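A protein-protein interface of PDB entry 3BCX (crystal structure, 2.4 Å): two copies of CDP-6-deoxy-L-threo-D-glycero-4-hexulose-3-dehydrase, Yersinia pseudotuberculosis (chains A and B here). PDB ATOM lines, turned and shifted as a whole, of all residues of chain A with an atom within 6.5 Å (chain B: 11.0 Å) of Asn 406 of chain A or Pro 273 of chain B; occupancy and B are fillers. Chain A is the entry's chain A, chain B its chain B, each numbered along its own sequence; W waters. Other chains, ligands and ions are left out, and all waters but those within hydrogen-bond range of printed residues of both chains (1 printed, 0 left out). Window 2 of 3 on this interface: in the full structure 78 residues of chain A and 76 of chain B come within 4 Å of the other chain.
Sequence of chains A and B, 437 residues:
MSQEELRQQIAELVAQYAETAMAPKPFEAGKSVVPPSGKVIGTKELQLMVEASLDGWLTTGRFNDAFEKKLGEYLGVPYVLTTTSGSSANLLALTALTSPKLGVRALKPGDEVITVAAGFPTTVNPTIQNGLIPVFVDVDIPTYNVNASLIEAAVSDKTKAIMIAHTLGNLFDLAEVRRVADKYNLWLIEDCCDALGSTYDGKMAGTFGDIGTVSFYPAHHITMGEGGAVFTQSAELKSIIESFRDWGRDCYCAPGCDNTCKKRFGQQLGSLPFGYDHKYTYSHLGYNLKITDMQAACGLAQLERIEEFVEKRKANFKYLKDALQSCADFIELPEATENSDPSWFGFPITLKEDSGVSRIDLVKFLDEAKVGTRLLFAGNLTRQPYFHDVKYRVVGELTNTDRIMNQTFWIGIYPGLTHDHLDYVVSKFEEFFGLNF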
ATOM      1  N   SER A 358      20.902 -28.569 -30.751  1.00  0.00           N
ATOM      2  CA  SER A 358      21.674 -27.646 -29.938  1.00  0.00           C
ATOM      3  C   SER A 358      22.998 -27.354 -30.623  1.00  0.00           C
ATOM      4  O   SER A 358      23.427 -28.106 -31.497  1.00  0.00           O
ATOM      5  CB  SER A 358      21.938 -28.273 -28.568  1.00  0.00           C
ATOM      6  OG  SER A 358      20.717 -28.550 -27.903  1.00  0.00           O
ATOM      7  N   ARG A 359      23.646 -26.267 -30.220  1.00  0.00           N
ATOM      8  CA  ARG A 359      24.935 -25.917 -30.796  1.00  0.00           C
ATOM      9  C   ARG A 359      25.932 -27.030 -30.481  1.00  0.00           C
ATOM     10  O   ARG A 359      26.854 -27.277 -31.260  1.00  0.00           O
ATOM     11  CB  ARG A 359      25.434 -24.582 -30.234  1.00  0.00           C
ATOM     12  CG  ARG A 359      26.747 -24.082 -30.854  1.00  0.00           C
ATOM     13  CD  ARG A 359      27.163 -22.780 -30.212  1.00  0.00           C
ATOM     14  NE  ARG A 359      27.222 -22.930 -28.761  1.00  0.00           N
ATOM     15  CZ  ARG A 359      27.201 -21.921 -27.896  1.00  0.00           C
ATOM     16  NH1 ARG A 359      27.126 -20.671 -28.329  1.00  0.00           N
ATOM     17  NH2 ARG A 359      27.243 -22.166 -26.591  1.00  0.00           N
ATOM     18  N   ILE A 360      25.736 -27.701 -29.345  1.00  0.00           N
ATOM     19  CA  ILE A 360      26.599 -28.803 -28.910  1.00  0.00           C
ATOM     20  C   ILE A 360      26.617 -29.927 -29.939  1.00  0.00           C
ATOM     21  O   ILE A 360      27.656 -30.535 -30.203  1.00  0.00           O
ATOM     22  CB  ILE A 360      26.109 -29.420 -27.571  1.00  0.00           C
ATOM     23  CG1 ILE A 360      26.235 -28.405 -26.443  1.00  0.00           C
ATOM     24  CG2 ILE A 360      26.937 -30.649 -27.225  1.00  0.00           C
ATOM     25  CD1 ILE A 360      27.674 -27.987 -26.185  1.00  0.00           C
ATOM     26  N   GLY A 379      31.212 -14.945 -24.865  1.00  0.00           N
ATOM     27  CA  GLY A 379      29.779 -15.130 -25.027  1.00  0.00           C
ATOM     28  C   GLY A 379      29.078 -13.932 -24.421  1.00  0.00           C
ATOM     29  O   GLY A 379      28.610 -13.046 -25.136  1.00  0.00           O
ATOM     30  N   ARG A 383      28.111 -12.976 -17.512  1.00  0.00           N
ATOM     31  CA  ARG A 383      27.756 -14.304 -17.019  1.00  0.00           C
ATOM     32  C   ARG A 383      28.984 -15.176 -16.732  1.00  0.00           C
ATOM     33  O   ARG A 383      28.852 -16.314 -16.278  1.00  0.00           O
ATOM     34  CB  ARG A 383      26.847 -15.020 -18.026  1.00  0.00           C
ATOM     35  CG  ARG A 383      25.524 -14.305 -18.286  1.00  0.00           C
ATOM     36  CD  ARG A 383      24.650 -15.112 -19.225  1.00  0.00           C
ATOM     37  NE  ARG A 383      23.369 -14.462 -19.468  1.00  0.00           N
ATOM     38  CZ  ARG A 383      22.368 -14.425 -18.593  1.00  0.00           C
ATOM     39  NH1 ARG A 383      22.494 -15.005 -17.405  1.00  0.00           N
ATOM     40  NH2 ARG A 383      21.237 -13.804 -18.910  1.00  0.00           N
ATOM     41  N   THR A 401      23.256 -10.663 -27.094  1.00  0.00           N
ATOM     42  CA  THR A 401      24.473 -11.125 -26.439  1.00  0.00           C
ATOM     43  C   THR A 401      24.251 -12.531 -25.894  1.00  0.00           C
ATOM     44  O   THR A 401      25.107 -13.406 -26.060  1.00  0.00           O
ATOM     45  CB  THR A 401      24.879 -10.196 -25.268  1.00  0.00           C
ATOM     46  OG1 THR A 401      25.064  -8.861 -25.755  1.00  0.00           O
ATOM     47  CG2 THR A 401      26.175 -10.678 -24.632  1.00  0.00           C
ATOM     48  N   ASP A 402      23.109 -12.748 -25.240  1.00  0.00           N
ATOM     49  CA  ASP A 402      22.793 -14.070 -24.692  1.00  0.00           C
ATOM     50  C   ASP A 402      22.537 -15.082 -25.806  1.00  0.00           C
ATOM     51  O   ASP A 402      22.816 -16.269 -25.655  1.00  0.00           O
ATOM     52  CB  ASP A 402      21.563 -14.022 -23.770  1.00  0.00           C
ATOM     53  CG  ASP A 402      21.913 -13.619 -22.338  1.00  0.00           C
ATOM     54  OD1 ASP A 402      23.061 -13.864 -21.896  1.00  0.00           O
ATOM     55  OD2 ASP A 402      21.030 -13.074 -21.644  1.00  0.00           O
ATOM     56  N   ARG A 403      22.000 -14.616 -26.924  1.00  0.00           N
ATOM     57  CA  ARG A 403      21.740 -15.518 -28.033  1.00  0.00           C
ATOM     58  C   ARG A 403      23.079 -15.999 -28.593  1.00  0.00           C
ATOM     59  O   ARG A 403      23.242 -17.174 -28.940  1.00  0.00           O
ATOM     60  CB  ARG A 403      20.938 -14.807 -29.122  1.00  0.00           C
ATOM     61  CG  ARG A 403      20.369 -15.763 -30.141  1.00  0.00           C
ATOM     62  CD  ARG A 403      19.614 -15.053 -31.242  1.00  0.00           C
ATOM     63  NE  ARG A 403      19.145 -16.021 -32.223  1.00  0.00           N
ATOM     64  CZ  ARG A 403      19.155 -15.821 -33.537  1.00  0.00           C
ATOM     65  NH1 ARG A 403      19.609 -14.683 -34.042  1.00  0.00           N
ATOM     66  NH2 ARG A 403      18.726 -16.778 -34.347  1.00  0.00           N
ATOM     67  N   ILE A 404      24.035 -15.077 -28.670  1.00  0.00           N
ATOM     68  CA  ILE A 404      25.374 -15.383 -29.166  1.00  0.00           C
ATOM     69  C   ILE A 404      25.988 -16.433 -28.253  1.00  0.00           C
ATOM     70  O   ILE A 404      26.490 -17.460 -28.711  1.00  0.00           O
ATOM     71  CB  ILE A 404      26.246 -14.089 -29.199  1.00  0.00           C
ATOM     72  CG1 ILE A 404      25.820 -13.228 -30.395  1.00  0.00           C
ATOM     73  CG2 ILE A 404      27.725 -14.428 -29.257  1.00  0.00           C
ATOM     74  CD1 ILE A 404      26.462 -11.856 -30.446  1.00  0.00           C
ATOM     75  N   MET A 405      25.905 -16.185 -26.951  1.00  0.00           N
ATOM     76  CA  MET A 405      26.448 -17.099 -25.954  1.00  0.00           C
ATOM     77  C   MET A 405      25.869 -18.506 -26.093  1.00  0.00           C
ATOM     78  O   MET A 405      26.573 -19.500 -25.878  1.00  0.00           O
ATOM     79  CB  MET A 405      26.159 -16.567 -24.545  1.00  0.00           C
ATOM     80  CG  MET A 405      26.636 -17.477 -23.418  1.00  0.00           C
ATOM     81  SD  MET A 405      26.038 -16.916 -21.818  1.00  0.00           S
ATOM     82  CE  MET A 405      24.289 -17.308 -21.970  1.00  0.00           C
ATOM     83  N   ASN A 406      24.591 -18.590 -26.459  1.00  0.00           N
ATOM     84  CA  ASN A 406      23.922 -19.883 -26.611  1.00  0.00           C
ATOM     85  C   ASN A 406      23.935 -20.507 -28.003  1.00  0.00           C
ATOM     86  O   ASN A 406      24.081 -21.719 -28.133  1.00  0.00           O
ATOM     87  CB  ASN A 406      22.451 -19.779 -26.183  1.00  0.00           C
ATOM     88  CG  ASN A 406      22.282 -19.544 -24.695  1.00  0.00           C
ATOM     89  OD1 ASN A 406      22.773 -20.316 -23.870  1.00  0.00           O
ATOM     90  ND2 ASN A 406      21.578 -18.471 -24.345  1.00  0.00           N
ATOM     91  N   GLN A 407      23.805 -19.685 -29.040  1.00  0.00           N
ATOM     92  CA  GLN A 407      23.694 -20.196 -30.407  1.00  0.00           C
ATOM     93  C   GLN A 407      24.785 -19.928 -31.438  1.00  0.00           C
ATOM     94  O   GLN A 407      24.748 -20.500 -32.533  1.00  0.00           O
ATOM     95  CB  GLN A 407      22.368 -19.696 -30.983  1.00  0.00           C
ATOM     96  CG  GLN A 407      21.161 -20.010 -30.105  1.00  0.00           C
ATOM     97  CD  GLN A 407      20.894 -21.496 -30.023  1.00  0.00           C
ATOM     98  OE1 GLN A 407      20.712 -22.158 -31.050  1.00  0.00           O
ATOM     99  NE2 GLN A 407      20.866 -22.034 -28.809  1.00  0.00           N
ATOM    100  N   THR A 408      25.750 -19.074 -31.109  1.00  0.00           N
ATOM    101  CA  THR A 408      26.792 -18.715 -32.066  1.00  0.00           C
ATOM    102  C   THR A 408      28.110 -19.451 -31.917  1.00  0.00           C
ATOM    103  O   THR A 408      28.452 -19.934 -30.843  1.00  0.00           O
ATOM    104  CB  THR A 408      27.082 -17.203 -31.997  1.00  0.00           C
ATOM    105  OG1 THR A 408      25.852 -16.478 -32.072  1.00  0.00           O
ATOM    106  CG2 THR A 408      27.979 -16.771 -33.144  1.00  0.00           C
ATOM    107  N   LEU B 269      30.100 -21.176 -10.694  1.00  0.00           N
ATOM    108  CA  LEU B 269      29.676 -19.780 -10.739  1.00  0.00           C
ATOM    109  C   LEU B 269      29.315 -19.311 -12.146  1.00  0.00           C
ATOM    110  O   LEU B 269      29.425 -20.069 -13.116  1.00  0.00           O
ATOM    111  CB  LEU B 269      30.768 -18.875 -10.172  1.00  0.00           C
ATOM    112  CG  LEU B 269      30.980 -18.944  -8.664  1.00  0.00           C
ATOM    113  CD1 LEU B 269      32.121 -18.023  -8.296  1.00  0.00           C
ATOM    114  CD2 LEU B 269      29.706 -18.533  -7.929  1.00  0.00           C
ATOM    115  N   GLY B 270      28.891 -18.055 -12.251  1.00  0.00           N
ATOM    116  CA  GLY B 270      28.507 -17.522 -13.544  1.00  0.00           C
ATOM    117  C   GLY B 270      27.256 -18.227 -14.033  1.00  0.00           C
ATOM    118  O   GLY B 270      26.811 -19.192 -13.420  1.00  0.00           O
ATOM    119  N   SER B 271      26.689 -17.760 -15.138  1.00  0.00           N
ATOM    120  CA  SER B 271      25.480 -18.360 -15.675  1.00  0.00           C
ATOM    121  C   SER B 271      25.639 -18.731 -17.139  1.00  0.00           C
ATOM    122  O   SER B 271      24.792 -18.398 -17.966  1.00  0.00           O
ATOM    123  CB  SER B 271      24.309 -17.396 -15.517  1.00  0.00           C
ATOM    124  OG  SER B 271      24.586 -16.160 -16.155  1.00  0.00           O
ATOM    125  N   LEU B 272      26.728 -19.419 -17.458  1.00  0.00           N
ATOM    126  CA  LEU B 272      26.989 -19.846 -18.828  1.00  0.00           C
ATOM    127  C   LEU B 272      26.211 -21.127 -19.134  1.00  0.00           C
ATOM    128  O   LEU B 272      26.020 -21.970 -18.252  1.00  0.00           O
ATOM    129  CB  LEU B 272      28.485 -20.106 -19.018  1.00  0.00           C
ATOM    130  CG  LEU B 272      29.431 -18.943 -18.727  1.00  0.00           C
ATOM    131  CD1 LEU B 272      30.863 -19.435 -18.824  1.00  0.00           C
ATOM    132  CD2 LEU B 272      29.173 -17.810 -19.712  1.00  0.00           C
ATOM    133  N   PRO B 273      25.767 -21.299 -20.391  1.00  0.00           N
ATOM    134  CA  PRO B 273      25.014 -22.500 -20.765  1.00  0.00           C
ATOM    135  C   PRO B 273      25.858 -23.765 -20.647  1.00  0.00           C
ATOM    136  O   PRO B 273      27.080 -23.724 -20.806  1.00  0.00           O
ATOM    137  CB  PRO B 273      24.607 -22.215 -22.209  1.00  0.00           C
ATOM    138  CG  PRO B 273      25.787 -21.436 -22.723  1.00  0.00           C
ATOM    139  CD  PRO B 273      26.060 -20.475 -21.578  1.00  0.00           C
ATOM    140  N   PHE B 274      25.200 -24.885 -20.369  1.00  0.00           N
ATOM    141  CA  PHE B 274      25.886 -26.167 -20.251  1.00  0.00           C
ATOM    142  C   PHE B 274      26.697 -26.476 -21.506  1.00  0.00           C
ATOM    143  O   PHE B 274      26.269 -26.180 -22.621  1.00  0.00           O
ATOM    144  CB  PHE B 274      24.881 -27.290 -19.984  1.00  0.00           C
ATOM    145  CG  PHE B 274      25.471 -28.667 -20.086  1.00  0.00           C
ATOM    146  CD1 PHE B 274      25.620 -29.283 -21.319  1.00  0.00           C
ATOM    147  CD2 PHE B 274      25.876 -29.348 -18.951  1.00  0.00           C
ATOM    148  CE1 PHE B 274      26.162 -30.550 -21.415  1.00  0.00           C
ATOM    149  CE2 PHE B 274      26.419 -30.616 -19.041  1.00  0.00           C
ATOM    150  CZ  PHE B 274      26.562 -31.217 -20.274  1.00  0.00           C
ATOM    151  N   GLY B 275      27.869 -27.073 -21.316  1.00  0.00           N
ATOM    152  CA  GLY B 275      28.729 -27.437 -22.426  1.00  0.00           C
ATOM    153  C   GLY B 275      29.264 -26.226 -23.165  1.00  0.00           C
ATOM    154  O   GLY B 275      29.496 -26.277 -24.373  1.00  0.00           O
ATOM    155  N   TYR B 276      29.460 -25.133 -22.436  1.00  0.00           N
ATOM    156  CA  TYR B 276      30.218 -23.997 -22.946  1.00  0.00           C
ATOM    157  C   TYR B 276      31.717 -24.274 -22.909  1.00  0.00           C
ATOM    158  O   TYR B 276      32.259 -24.676 -21.879  1.00  0.00           O
ATOM    159  CB  TYR B 276      29.896 -22.733 -22.144  1.00  0.00           C
ATOM    160  CG  TYR B 276      30.175 -21.448 -22.890  1.00  0.00           C
ATOM    161  CD1 TYR B 276      29.254 -20.932 -23.792  1.00  0.00           C
ATOM    162  CD2 TYR B 276      31.359 -20.750 -22.693  1.00  0.00           C
ATOM    163  CE1 TYR B 276      29.504 -19.758 -24.476  1.00  0.00           C
ATOM    164  CE2 TYR B 276      31.618 -19.576 -23.371  1.00  0.00           C
ATOM    165  CZ  TYR B 276      30.688 -19.083 -24.262  1.00  0.00           C
ATOM    166  OH  TYR B 276      30.942 -17.913 -24.940  1.00  0.00           O
ATOM    167  N   ASP B 277      32.382 -24.055 -24.039  1.00  0.00           N
ATOM    168  CA  ASP B 277      33.801 -24.374 -24.169  1.00  0.00           C
ATOM    169  C   ASP B 277      34.587 -23.967 -22.924  1.00  0.00           C
ATOM    170  O   ASP B 277      34.578 -22.797 -22.536  1.00  0.00           O
ATOM    171  CB  ASP B 277      34.380 -23.662 -25.397  1.00  0.00           C
ATOM    172  CG  ASP B 277      35.619 -24.351 -25.944  1.00  0.00           C
ATOM    173  OD1 ASP B 277      36.557 -24.614 -25.161  1.00  0.00           O
ATOM    174  OD2 ASP B 277      35.655 -24.627 -27.163  1.00  0.00           O
ATOM    175  N   HIS B 278      35.265 -24.928 -22.299  1.00  0.00           N
ATOM    176  CA  HIS B 278      36.044 -24.616 -21.105  1.00  0.00           C
ATOM    177  C   HIS B 278      37.173 -23.646 -21.456  1.00  0.00           C
ATOM    178  O   HIS B 278      37.584 -22.838 -20.627  1.00  0.00           O
ATOM    179  CB  HIS B 278      36.646 -25.881 -20.478  1.00  0.00           C
ATOM    180  CG  HIS B 278      37.066 -25.700 -19.048  1.00  0.00           C
ATOM    181  ND1 HIS B 278      38.099 -26.412 -18.475  1.00  0.00           N
ATOM    182  CD2 HIS B 278      36.564 -24.910 -18.067  1.00  0.00           C
ATOM    183  CE1 HIS B 278      38.217 -26.068 -17.203  1.00  0.00           C
ATOM    184  NE2 HIS B 278      37.297 -25.159 -16.930  1.00  0.00           N
ATOM    185  N   LYS B 279      37.668 -23.731 -22.688  1.00  0.00           N
ATOM    186  CA  LYS B 279      38.751 -22.861 -23.144  1.00  0.00           C
ATOM    187  C   LYS B 279      38.321 -21.399 -23.123  1.00  0.00           C
ATOM    188  O   LYS B 279      39.161 -20.497 -23.116  1.00  0.00           O
ATOM    189  CB  LYS B 279      39.190 -23.248 -24.563  1.00  0.00           C
ATOM    190  CG  LYS B 279      39.679 -24.692 -24.696  1.00  0.00           C
ATOM    191  CD  LYS B 279      40.917 -24.966 -23.838  1.00  0.00           C
ATOM    192  CE  LYS B 279      42.133 -24.192 -24.340  1.00  0.00           C
ATOM    193  NZ  LYS B 279      42.482 -24.546 -25.749  1.00  0.00           N
ATOM    194  N   TYR B 280      37.011 -21.175 -23.106  1.00  0.00           N
ATOM    195  CA  TYR B 280      36.461 -19.823 -23.080  1.00  0.00           C
ATOM    196  C   TYR B 280      35.660 -19.548 -21.805  1.00  0.00           C
ATOM    197  O   TYR B 280      34.675 -18.808 -21.815  1.00  0.00           O
ATOM    198  CB  TYR B 280      35.589 -19.577 -24.317  1.00  0.00           C
ATOM    199  CG  TYR B 280      36.364 -19.374 -25.605  1.00  0.00           C
ATOM    200  CD1 TYR B 280      35.699 -19.299 -26.830  1.00  0.00           C
ATOM    201  CD2 TYR B 280      37.754 -19.225 -25.601  1.00  0.00           C
ATOM    202  CE1 TYR B 280      36.395 -19.076 -28.020  1.00  0.00           C
ATOM    203  CE2 TYR B 280      38.463 -19.001 -26.787  1.00  0.00           C
ATOM    204  CZ  TYR B 280      37.774 -18.927 -27.993  1.00  0.00           C
ATOM    205  OH  TYR B 280      38.451 -18.695 -29.168  1.00  0.00           O
ATOM    206  N   THR B 281      36.095 -20.155 -20.705  1.00  0.00           N
ATOM    207  CA  THR B 281      35.488 -19.907 -19.403  1.00  0.00           C
ATOM    208  C   THR B 281      36.504 -19.331 -18.422  1.00  0.00           C
ATOM    209  O   THR B 281      37.554 -19.926 -18.181  1.00  0.00           O
ATOM    210  CB  THR B 281      34.886 -21.193 -18.807  1.00  0.00           C
ATOM    211  OG1 THR B 281      33.864 -21.693 -19.678  1.00  0.00           O
ATOM    212  CG2 THR B 281      34.288 -20.917 -17.436  1.00  0.00           C
HETATM  213  O   HOH W   1      26.715 -24.702 -25.169  1.00  0.00           O
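Of the 13 printed residues of chain A, 6 touch a printed residue of chain B. Among the printed residues, 10 pairs touch across the chains. Among the printed residues, no Asp or Glu carboxylate lies within 4 Å of a Lys or Arg side-chain nitrogen of the other chain.
No position is printed for both chains. Of the 10 pairs that touch across the chains among the printed residues, none has its exchanged pair printed and touching as well.
Of the printed residues of chain B, Arg 359 of chain A touches Tyr 276. Of the printed residues of chain B, Gly 379 of chain A touches Tyr 276 (3.0 Å). Of the printed residues of chain B, Arg 383 of chain A touches Gly 270, Ser 271 and Leu 272. Of the printed residues of chain B, Met 405 of chain A touches Leu 272 (3.9 Å), Pro 273 (3.6 Å) and Tyr 276 (3.3 Å). Asn 406 of chain A touches just one residue of chain B: Pro 273 (3.1 Å). No residue of chain B comes within 4 Å of Gln 407 of chain A. Thr 408 of chain A touches none of the printed residues of chain B. Printed residues of chain A within 4 Å of Pro 273 of chain B: Met 405 (3.6 Å) and Asn 406 (3.1 Å). Of the printed residues of chain A, Tyr 276 of chain B touches Arg 359 (3.7 Å), Gly 379 (3.0 Å) and Met 405 (3.3 Å). Asp 277 of chain B touches none of the printed residues of chain A. The nearest printed residue of chain B that does not touch Arg 383 of chain A is Leu 269 of chain B (4.9 Å).
Water W1 lies within hydrogen-bond range of NH2 of Arg 359 of chain A (3.0 Å), O of Phe 274 of chain B (3.0 Å) and O of Gly 275 of chain B (3.3 Å).
O of Asp 402 of chain A is in hydrogen-bond range of ND2 of Asn 406 of chain A. The guanidinium group (NH1) of Arg 359 of chain A is in hydrogen-bond range of the backbone carbonyl oxygen (O) of Met 405 of chain A (2.8 Å). The side-chain carboxylate (OD1) of Asp 402 of chain A lies within salt-bridge range of the guanidinium group (NE) of Arg 383 of chain A (2.5 Å). The guanidinium group (NH1) of Arg 359 of chain A sits close to the backbone carbonyl oxygen (O) of Asn 406 of chain A (3.2 Å). The guanidinium group (NH1) of Arg 359 of chain A lies within hydrogen-bond range of the backbone carbonyl oxygen (O) of Thr 408 of chain A (2.9 Å). The guanidinium group of Arg 359 of chain A is in hydrogen-bond range of the backbone carbonyl oxygen of Ile 404 of chain A, at 3.3 Å.
Among the printed residues, merely in contact across the chains: Arg 383 of chain A with Gly 270 of chain B, Ile 360 of chain A with Gly 275 of chain B, Asn 406 of chain A with Pro 273 of chain B, Met 405 of chain A with Tyr 276 of chain B, Met 405 of chain A with Pro 273 of chain B, Arg 383 of chain A with Leu 272 of chain B, Arg 359 of chain A with Tyr 276 of chain B and Met 405 of chain A with Leu 272 of chain B.
N of Gly 379 of chain A lies within hydrogen-bond range of OH of Tyr 276 of chain B. The guanidinium group (NH1) of Arg 383 of chain A is in hydrogen-bond range of the side-chain hydroxyl (OG) of Ser 271 of chain B.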
